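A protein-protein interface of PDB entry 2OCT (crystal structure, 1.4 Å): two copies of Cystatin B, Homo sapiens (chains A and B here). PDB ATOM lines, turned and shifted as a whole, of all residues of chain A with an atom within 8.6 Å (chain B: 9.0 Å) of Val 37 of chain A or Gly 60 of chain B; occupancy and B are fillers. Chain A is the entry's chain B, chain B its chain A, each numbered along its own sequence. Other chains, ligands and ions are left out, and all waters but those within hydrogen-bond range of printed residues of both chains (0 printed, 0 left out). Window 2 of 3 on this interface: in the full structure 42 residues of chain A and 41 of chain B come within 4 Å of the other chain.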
ATOM      1  N   GLN A  17      -7.881 -29.865  12.792  1.00  0.00           N
ATOM      2  CA  GLN A  17      -9.045 -29.729  13.674  1.00  0.00           C
ATOM      3  C   GLN A  17      -8.738 -30.291  15.051  1.00  0.00           C
ATOM      4  O   GLN A  17      -9.152 -29.685  16.056  1.00  0.00           O
ATOM      5  CB  GLN A  17     -10.257 -30.457  13.121  1.00  0.00           C
ATOM      6  CG  GLN A  17     -11.538 -30.213  13.889  1.00  0.00           C
ATOM      7  CD  GLN A  17     -11.911 -28.729  13.918  1.00  0.00           C
ATOM      8  OE1 GLN A  17     -12.008 -28.100  12.860  1.00  0.00           O
ATOM      9  NE2 GLN A  17     -12.131 -28.195  15.118  1.00  0.00           N
ATOM     10  N   ALA A  20      -6.942 -27.584  16.727  1.00  0.00           N
ATOM     11  CA  ALA A  20      -7.876 -26.524  17.095  1.00  0.00           C
ATOM     12  C   ALA A  20      -8.733 -26.925  18.279  1.00  0.00           C
ATOM     13  O   ALA A  20      -9.010 -26.054  19.112  1.00  0.00           O
ATOM     14  CB  ALA A  20      -8.735 -26.162  15.874  1.00  0.00           C
ATOM     15  N   ASP A  21      -9.187 -28.172  18.353  1.00  0.00           N
ATOM     16  CA  ASP A  21     -10.007 -28.583  19.512  1.00  0.00           C
ATOM     17  C   ASP A  21      -9.256 -28.415  20.832  1.00  0.00           C
ATOM     18  O   ASP A  21      -9.827 -27.972  21.840  1.00  0.00           O
ATOM     19  CB  ASP A  21     -10.400 -30.046  19.391  1.00  0.00           C
ATOM     20  CG  ASP A  21     -11.256 -30.406  18.198  1.00  0.00           C
ATOM     21  OD1 ASP A  21     -11.987 -29.537  17.686  1.00  0.00           O
ATOM     22  OD2 ASP A  21     -11.188 -31.612  17.803  1.00  0.00           O
ATOM     23  N   ARG A  24      -9.027 -24.707  21.613  1.00  0.00           N
ATOM     24  CA  ARG A  24     -10.293 -24.160  22.129  1.00  0.00           C
ATOM     25  C   ARG A  24     -10.378 -24.313  23.637  1.00  0.00           C
ATOM     26  O   ARG A  24     -10.780 -23.405  24.392  1.00  0.00           O
ATOM     27  CB  ARG A  24     -11.443 -24.862  21.437  1.00  0.00           C
ATOM     28  CG  ARG A  24     -12.808 -24.284  21.801  1.00  0.00           C
ATOM     29  CD  ARG A  24     -13.909 -25.168  21.202  1.00  0.00           C
ATOM     30  NE  ARG A  24     -15.208 -24.454  21.269  1.00  0.00           N
ATOM     31  CZ  ARG A  24     -16.305 -25.051  20.800  1.00  0.00           C
ATOM     32  NH1 ARG A  24     -16.288 -26.283  20.240  1.00  0.00           N
ATOM     33  NH2 ARG A  24     -17.482 -24.415  20.863  1.00  0.00           N
ATOM     34  N   LYS A  34     -14.676 -17.899  25.117  1.00  0.00           N
ATOM     35  CA  LYS A  34     -15.618 -18.941  24.708  1.00  0.00           C
ATOM     36  C   LYS A  34     -16.108 -18.687  23.295  1.00  0.00           C
ATOM     37  O   LYS A  34     -16.301 -17.510  22.945  1.00  0.00           O
ATOM     38  CB  LYS A  34     -16.764 -18.899  25.722  1.00  0.00           C
ATOM     39  CG  LYS A  34     -16.353 -19.215  27.164  1.00  0.00           C
ATOM     40  CD  LYS A  34     -17.587 -19.426  28.035  1.00  0.00           C
ATOM     41  CE  LYS A  34     -18.253 -18.084  28.300  1.00  0.00           C
ATOM     42  NZ  LYS A  34     -17.391 -17.282  29.215  1.00  0.00           N
ATOM     43  N   PHE A  35     -16.348 -19.725  22.499  1.00  0.00           N
ATOM     44  CA  PHE A  35     -16.876 -19.557  21.138  1.00  0.00           C
ATOM     45  C   PHE A  35     -17.991 -20.572  20.884  1.00  0.00           C
ATOM     46  O   PHE A  35     -17.948 -21.649  21.475  1.00  0.00           O
ATOM     47  CB  PHE A  35     -15.793 -19.769  20.085  1.00  0.00           C
ATOM     48  CG  PHE A  35     -14.547 -18.929  20.298  1.00  0.00           C
ATOM     49  CD1 PHE A  35     -14.493 -17.606  19.866  1.00  0.00           C
ATOM     50  CD2 PHE A  35     -13.443 -19.461  20.938  1.00  0.00           C
ATOM     51  CE1 PHE A  35     -13.368 -16.810  20.067  1.00  0.00           C
ATOM     52  CE2 PHE A  35     -12.346 -18.640  21.148  1.00  0.00           C
ATOM     53  CZ  PHE A  35     -12.300 -17.316  20.748  1.00  0.00           C
ATOM     54  N   PRO A  36     -18.944 -20.269  20.044  1.00  0.00           N
ATOM     55  CA  PRO A  36     -20.013 -21.224  19.759  1.00  0.00           C
ATOM     56  C   PRO A  36     -19.580 -22.349  18.807  1.00  0.00           C
ATOM     57  O   PRO A  36     -20.223 -23.405  18.831  1.00  0.00           O
ATOM     58  CB  PRO A  36     -21.094 -20.378  19.058  1.00  0.00           C
ATOM     59  CG  PRO A  36     -20.344 -19.221  18.506  1.00  0.00           C
ATOM     60  CD  PRO A  36     -19.134 -18.970  19.365  1.00  0.00           C
ATOM     61  N   VAL A  37     -18.509 -22.128  18.053  1.00  0.00           N
ATOM     62  CA  VAL A  37     -17.945 -23.167  17.181  1.00  0.00           C
ATOM     63  C   VAL A  37     -16.462 -22.881  17.054  1.00  0.00           C
ATOM     64  O   VAL A  37     -16.027 -21.779  17.397  1.00  0.00           O
ATOM     65  CB  VAL A  37     -18.595 -23.203  15.795  1.00  0.00           C
ATOM     66  CG1 VAL A  37     -18.194 -22.017  14.926  1.00  0.00           C
ATOM     67  CG2 VAL A  37     -18.304 -24.501  15.058  1.00  0.00           C
ATOM     68  N   PHE A  38     -15.695 -23.872  16.600  1.00  0.00           N
ATOM     69  CA  PHE A  38     -14.249 -23.641  16.532  1.00  0.00           C
ATOM     70  C   PHE A  38     -13.711 -24.532  15.417  1.00  0.00           C
ATOM     71  O   PHE A  38     -13.061 -25.551  15.660  1.00  0.00           O
ATOM     72  CB  PHE A  38     -13.592 -23.917  17.876  1.00  0.00           C
ATOM     73  CG  PHE A  38     -12.285 -23.157  18.125  1.00  0.00           C
ATOM     74  CD1 PHE A  38     -12.317 -21.807  18.478  1.00  0.00           C
ATOM     75  CD2 PHE A  38     -11.062 -23.796  18.006  1.00  0.00           C
ATOM     76  CE1 PHE A  38     -11.125 -21.144  18.691  1.00  0.00           C
ATOM     77  CE2 PHE A  38      -9.870 -23.145  18.211  1.00  0.00           C
ATOM     78  CZ  PHE A  38      -9.886 -21.800  18.544  1.00  0.00           C
ATOM     79  N   LYS A  39     -13.989 -24.163  14.168  1.00  0.00           N
ATOM     80  CA  LYS A  39     -13.747 -25.025  13.021  1.00  0.00           C
ATOM     81  C   LYS A  39     -12.553 -24.584  12.185  1.00  0.00           C
ATOM     82  O   LYS A  39     -12.560 -23.531  11.542  1.00  0.00           O
ATOM     83  CB  LYS A  39     -14.996 -25.074  12.126  1.00  0.00           C
ATOM     84  CG  LYS A  39     -14.738 -25.729  10.764  1.00  0.00           C
ATOM     85  CD  LYS A  39     -16.026 -25.760   9.956  1.00  0.00           C
ATOM     86  CE  LYS A  39     -15.934 -26.612   8.709  1.00  0.00           C
ATOM     87  NZ  LYS A  39     -16.385 -25.878   7.492  1.00  0.00           N
ATOM     88  N   ALA A  40     -11.534 -25.436  12.177  1.00  0.00           N
ATOM     89  CA  ALA A  40     -10.299 -25.126  11.457  1.00  0.00           C
ATOM     90  C   ALA A  40     -10.633 -24.988   9.973  1.00  0.00           C
ATOM     91  O   ALA A  40     -11.367 -25.855   9.458  1.00  0.00           O
ATOM     92  CB  ALA A  40      -9.272 -26.201  11.758  1.00  0.00           C
ATOM     93  N   VAL B  57      -9.313 -20.188  11.946  1.00  0.00           N
ATOM     94  CA  VAL B  57     -10.417 -20.948  12.562  1.00  0.00           C
ATOM     95  C   VAL B  57     -11.709 -20.158  12.458  1.00  0.00           C
ATOM     96  O   VAL B  57     -11.693 -18.969  12.774  1.00  0.00           O
ATOM     97  CB  VAL B  57     -10.095 -21.214  14.053  1.00  0.00           C
ATOM     98  CG1 VAL B  57     -11.236 -21.930  14.758  1.00  0.00           C
ATOM     99  CG2 VAL B  57      -8.809 -21.993  14.215  1.00  0.00           C
ATOM    100  N   HIS B  58     -12.792 -20.770  12.003  1.00  0.00           N
ATOM    101  CA  HIS B  58     -14.107 -20.127  12.006  1.00  0.00           C
ATOM    102  C   HIS B  58     -14.783 -20.268  13.378  1.00  0.00           C
ATOM    103  O   HIS B  58     -14.890 -21.387  13.904  1.00  0.00           O
ATOM    104  CB  HIS B  58     -14.997 -20.729  10.925  1.00  0.00           C
ATOM    105  CG  HIS B  58     -16.360 -20.130  10.885  1.00  0.00           C
ATOM    106  ND1 HIS B  58     -17.511 -20.878  10.936  1.00  0.00           N
ATOM    107  CD2 HIS B  58     -16.708 -18.834  10.772  1.00  0.00           C
ATOM    108  CE1 HIS B  58     -18.555 -20.043  10.867  1.00  0.00           C
ATOM    109  NE2 HIS B  58     -18.084 -18.803  10.767  1.00  0.00           N
ATOM    110  N   VAL B  59     -15.197 -19.118  13.927  1.00  0.00           N
ATOM    111  CA  VAL B  59     -15.836 -19.197  15.258  1.00  0.00           C
ATOM    112  C   VAL B  59     -17.285 -18.718  15.218  1.00  0.00           C
ATOM    113  O   VAL B  59     -17.845 -18.378  16.263  1.00  0.00           O
ATOM    114  CB  VAL B  59     -15.002 -18.474  16.336  1.00  0.00           C
ATOM    115  CG1 VAL B  59     -13.610 -19.125  16.427  1.00  0.00           C
ATOM    116  CG2 VAL B  59     -14.839 -16.990  16.093  1.00  0.00           C
ATOM    117  N   GLY B  60     -17.886 -18.764  14.029  1.00  0.00           N
ATOM    118  CA  GLY B  60     -19.308 -18.565  13.840  1.00  0.00           C
ATOM    119  C   GLY B  60     -19.591 -17.264  13.131  1.00  0.00           C
ATOM    120  O   GLY B  60     -18.816 -16.306  13.230  1.00  0.00           O
ATOM    121  N   ASP B  61     -20.685 -17.230  12.402  1.00  0.00           N
ATOM    122  CA  ASP B  61     -21.055 -16.082  11.570  1.00  0.00           C
ATOM    123  C   ASP B  61     -19.872 -15.630  10.725  1.00  0.00           C
ATOM    124  O   ASP B  61     -19.293 -16.446   9.992  1.00  0.00           O
ATOM    125  CB  ASP B  61     -21.629 -14.965  12.453  1.00  0.00           C
ATOM    126  CG  ASP B  61     -22.910 -15.459  13.108  1.00  0.00           C
ATOM    127  OD1 ASP B  61     -23.685 -16.204  12.471  1.00  0.00           O
ATOM    128  OD2 ASP B  61     -23.153 -15.116  14.277  1.00  0.00           O
ATOM    129  N   GLU B  62     -19.477 -14.359  10.775  1.00  0.00           N
ATOM    130  CA  GLU B  62     -18.355 -13.919   9.935  1.00  0.00           C
ATOM    131  C   GLU B  62     -17.080 -13.791  10.773  1.00  0.00           C
ATOM    132  O   GLU B  62     -16.139 -13.120  10.350  1.00  0.00           O
ATOM    133  CB  GLU B  62     -18.636 -12.585   9.258  1.00  0.00           C
ATOM    134  CG  GLU B  62     -19.836 -12.560   8.319  1.00  0.00           C
ATOM    135  CD  GLU B  62     -20.140 -11.201   7.732  1.00  0.00           C
ATOM    136  OE1 GLU B  62     -20.422 -11.129   6.513  1.00  0.00           O
ATOM    137  OE2 GLU B  62     -20.119 -10.163   8.439  1.00  0.00           O
ATOM    138  N   ASP B  63     -17.089 -14.419  11.939  1.00  0.00           N
ATOM    139  CA  ASP B  63     -16.002 -14.254  12.900  1.00  0.00           C
ATOM    140  C   ASP B  63     -14.955 -15.349  12.818  1.00  0.00           C
ATOM    141  O   ASP B  63     -15.308 -16.519  12.732  1.00  0.00           O
ATOM    142  CB  ASP B  63     -16.535 -14.256  14.343  1.00  0.00           C
ATOM    143  CG  ASP B  63     -17.466 -13.107  14.659  1.00  0.00           C
ATOM    144  OD1 ASP B  63     -17.163 -11.965  14.258  1.00  0.00           O
ATOM    145  OD2 ASP B  63     -18.509 -13.329  15.324  1.00  0.00           O
ATOM    146  N   PHE B  64     -13.682 -14.949  12.834  1.00  0.00           N
ATOM    147  CA  PHE B  64     -12.591 -15.896  12.755  1.00  0.00           C
ATOM    148  C   PHE B  64     -11.551 -15.638  13.844  1.00  0.00           C
ATOM    149  O   PHE B  64     -11.465 -14.560  14.411  1.00  0.00           O
ATOM    150  CB  PHE B  64     -11.932 -15.810  11.353  1.00  0.00           C
ATOM    151  CG  PHE B  64     -12.841 -16.335  10.251  1.00  0.00           C
ATOM    152  CD1 PHE B  64     -13.876 -15.563   9.730  1.00  0.00           C
ATOM    153  CD2 PHE B  64     -12.689 -17.613   9.738  1.00  0.00           C
ATOM    154  CE1 PHE B  64     -14.720 -16.054   8.767  1.00  0.00           C
ATOM    155  CE2 PHE B  64     -13.501 -18.101   8.747  1.00  0.00           C
ATOM    156  CZ  PHE B  64     -14.525 -17.316   8.242  1.00  0.00           C
ATOM    157  N   VAL B  65     -10.748 -16.671  14.112  1.00  0.00           N
ATOM    158  CA  VAL B  65      -9.593 -16.582  15.014  1.00  0.00           C
ATOM    159  C   VAL B  65      -8.366 -17.062  14.258  1.00  0.00           C
ATOM    160  O   VAL B  65      -8.511 -18.024  13.493  1.00  0.00           O
ATOM    161  CB  VAL B  65      -9.847 -17.381  16.302  1.00  0.00           C
ATOM    162  CG1 VAL B  65      -8.616 -17.482  17.191  1.00  0.00           C
ATOM    163  CG2 VAL B  65     -10.993 -16.711  17.088  1.00  0.00           C
ATOM    164  N   LYS B  89     -10.954 -11.799  13.442  1.00  0.00           N
ATOM    165  CA  LYS B  89     -10.416 -11.861  12.084  1.00  0.00           C
ATOM    166  C   LYS B  89     -11.507 -12.170  11.075  1.00  0.00           C
ATOM    167  O   LYS B  89     -12.627 -12.584  11.393  1.00  0.00           O
ATOM    168  CB  LYS B  89      -9.313 -12.918  12.055  1.00  0.00           C
ATOM    169  CG  LYS B  89      -8.458 -13.015  13.314  1.00  0.00           C
ATOM    170  CD  LYS B  89      -7.771 -11.722  13.703  1.00  0.00           C
ATOM    171  CE  LYS B  89      -6.486 -11.494  12.946  1.00  0.00           C
ATOM    172  NZ  LYS B  89      -6.497 -12.034  11.569  1.00  0.00           N
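Arg 24 of chain A touches none of the printed residues of chain B. Lys 34 of chain A touches none of the printed residues of chain B. Printed residues of chain B within 4 Å of Val 37 of chain A: His 58 (3.5 Å), Val 59 (3.4 Å) and Gly 60 (3.4 Å). Of the printed residues of chain B, Phe 38 of chain A touches Val 57, His 58 and Val 59. Of the printed residues of chain A, His 58 of chain B touches Val 37 (3.5 Å), Phe 38 (3.5 Å) and Lys 39 (2.8 Å). Val 59 of chain B touches four residues of chain A. Gly 60 of chain B touches just one residue of chain A: Val 37 (3.4 Å). No residue of chain A comes within 4 Å of Asp 61 of chain B. The nearest residue of chain A that does not touch Gly 60 of chain B is Pro 36 of chain A (4.8 Å).
N of His 58 of chain B lies within hydrogen-bond range of O of Lys 39 of chain A (2.8 Å).
N of Val 57 of chain B lies within hydrogen-bond range of O of Val 65 of chain B, at 2.8 Å. The guanidinium group (NH2) of Arg 24 of chain A is in hydrogen-bond range of the backbone carbonyl oxygen (O) of Phe 35 of chain A (2.9 Å). A ring nitrogen (NE2) of His 58 of chain B sits at hydrogen-bond distance from the backbone carbonyl oxygen of Asp 61 of chain B. The backbone carbonyl oxygen (O) of Phe 38 of chain A is in hydrogen-bond range of the side-chain amide nitrogen (NE2) of Gln 17 of chain A, at 2.9 Å. A ring nitrogen (NE2) of His 58 of chain B sits close to the backbone NH (N) of Gly 60 of chain B, at 3.3 Å.
Hydrophobic or aromatic side chains of chain A within 4 Å of the printed part of chain B: Phe 35, Pro 36, Val 37 and Phe 38. Among the printed residues, 11 pairs touch across the chains.
No position is printed for both chains. Of the 11 pairs that touch across the chains among the printed residues, none has its exchanged pair printed and touching as well.
Among the printed residues, pairs that only touch across the chains: Phe 35 of chain A with Val 59 of chain B (3.7 Å), Phe 35 of chain A with Val 65 of chain B (3.8 Å), Pro 36 of chain A with Val 59 of chain B (3.4 Å), Val 37 of chain A with His 58 of chain B (3.5 Å), Val 37 of chain A with Val 59 of chain B (3.4 Å), Val 37 of chain A with Gly 60 of chain B (3.4 Å), Phe 38 of chain A with Val 57 of chain B (3.7 Å), Phe 38 of chain A with His 58 of chain B (3.5 Å), Phe 38 of chain A with Val 59 of chain B (3.6 Å) and Lys 39 of chain A with Val 57 of chain B (3.5 Å).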
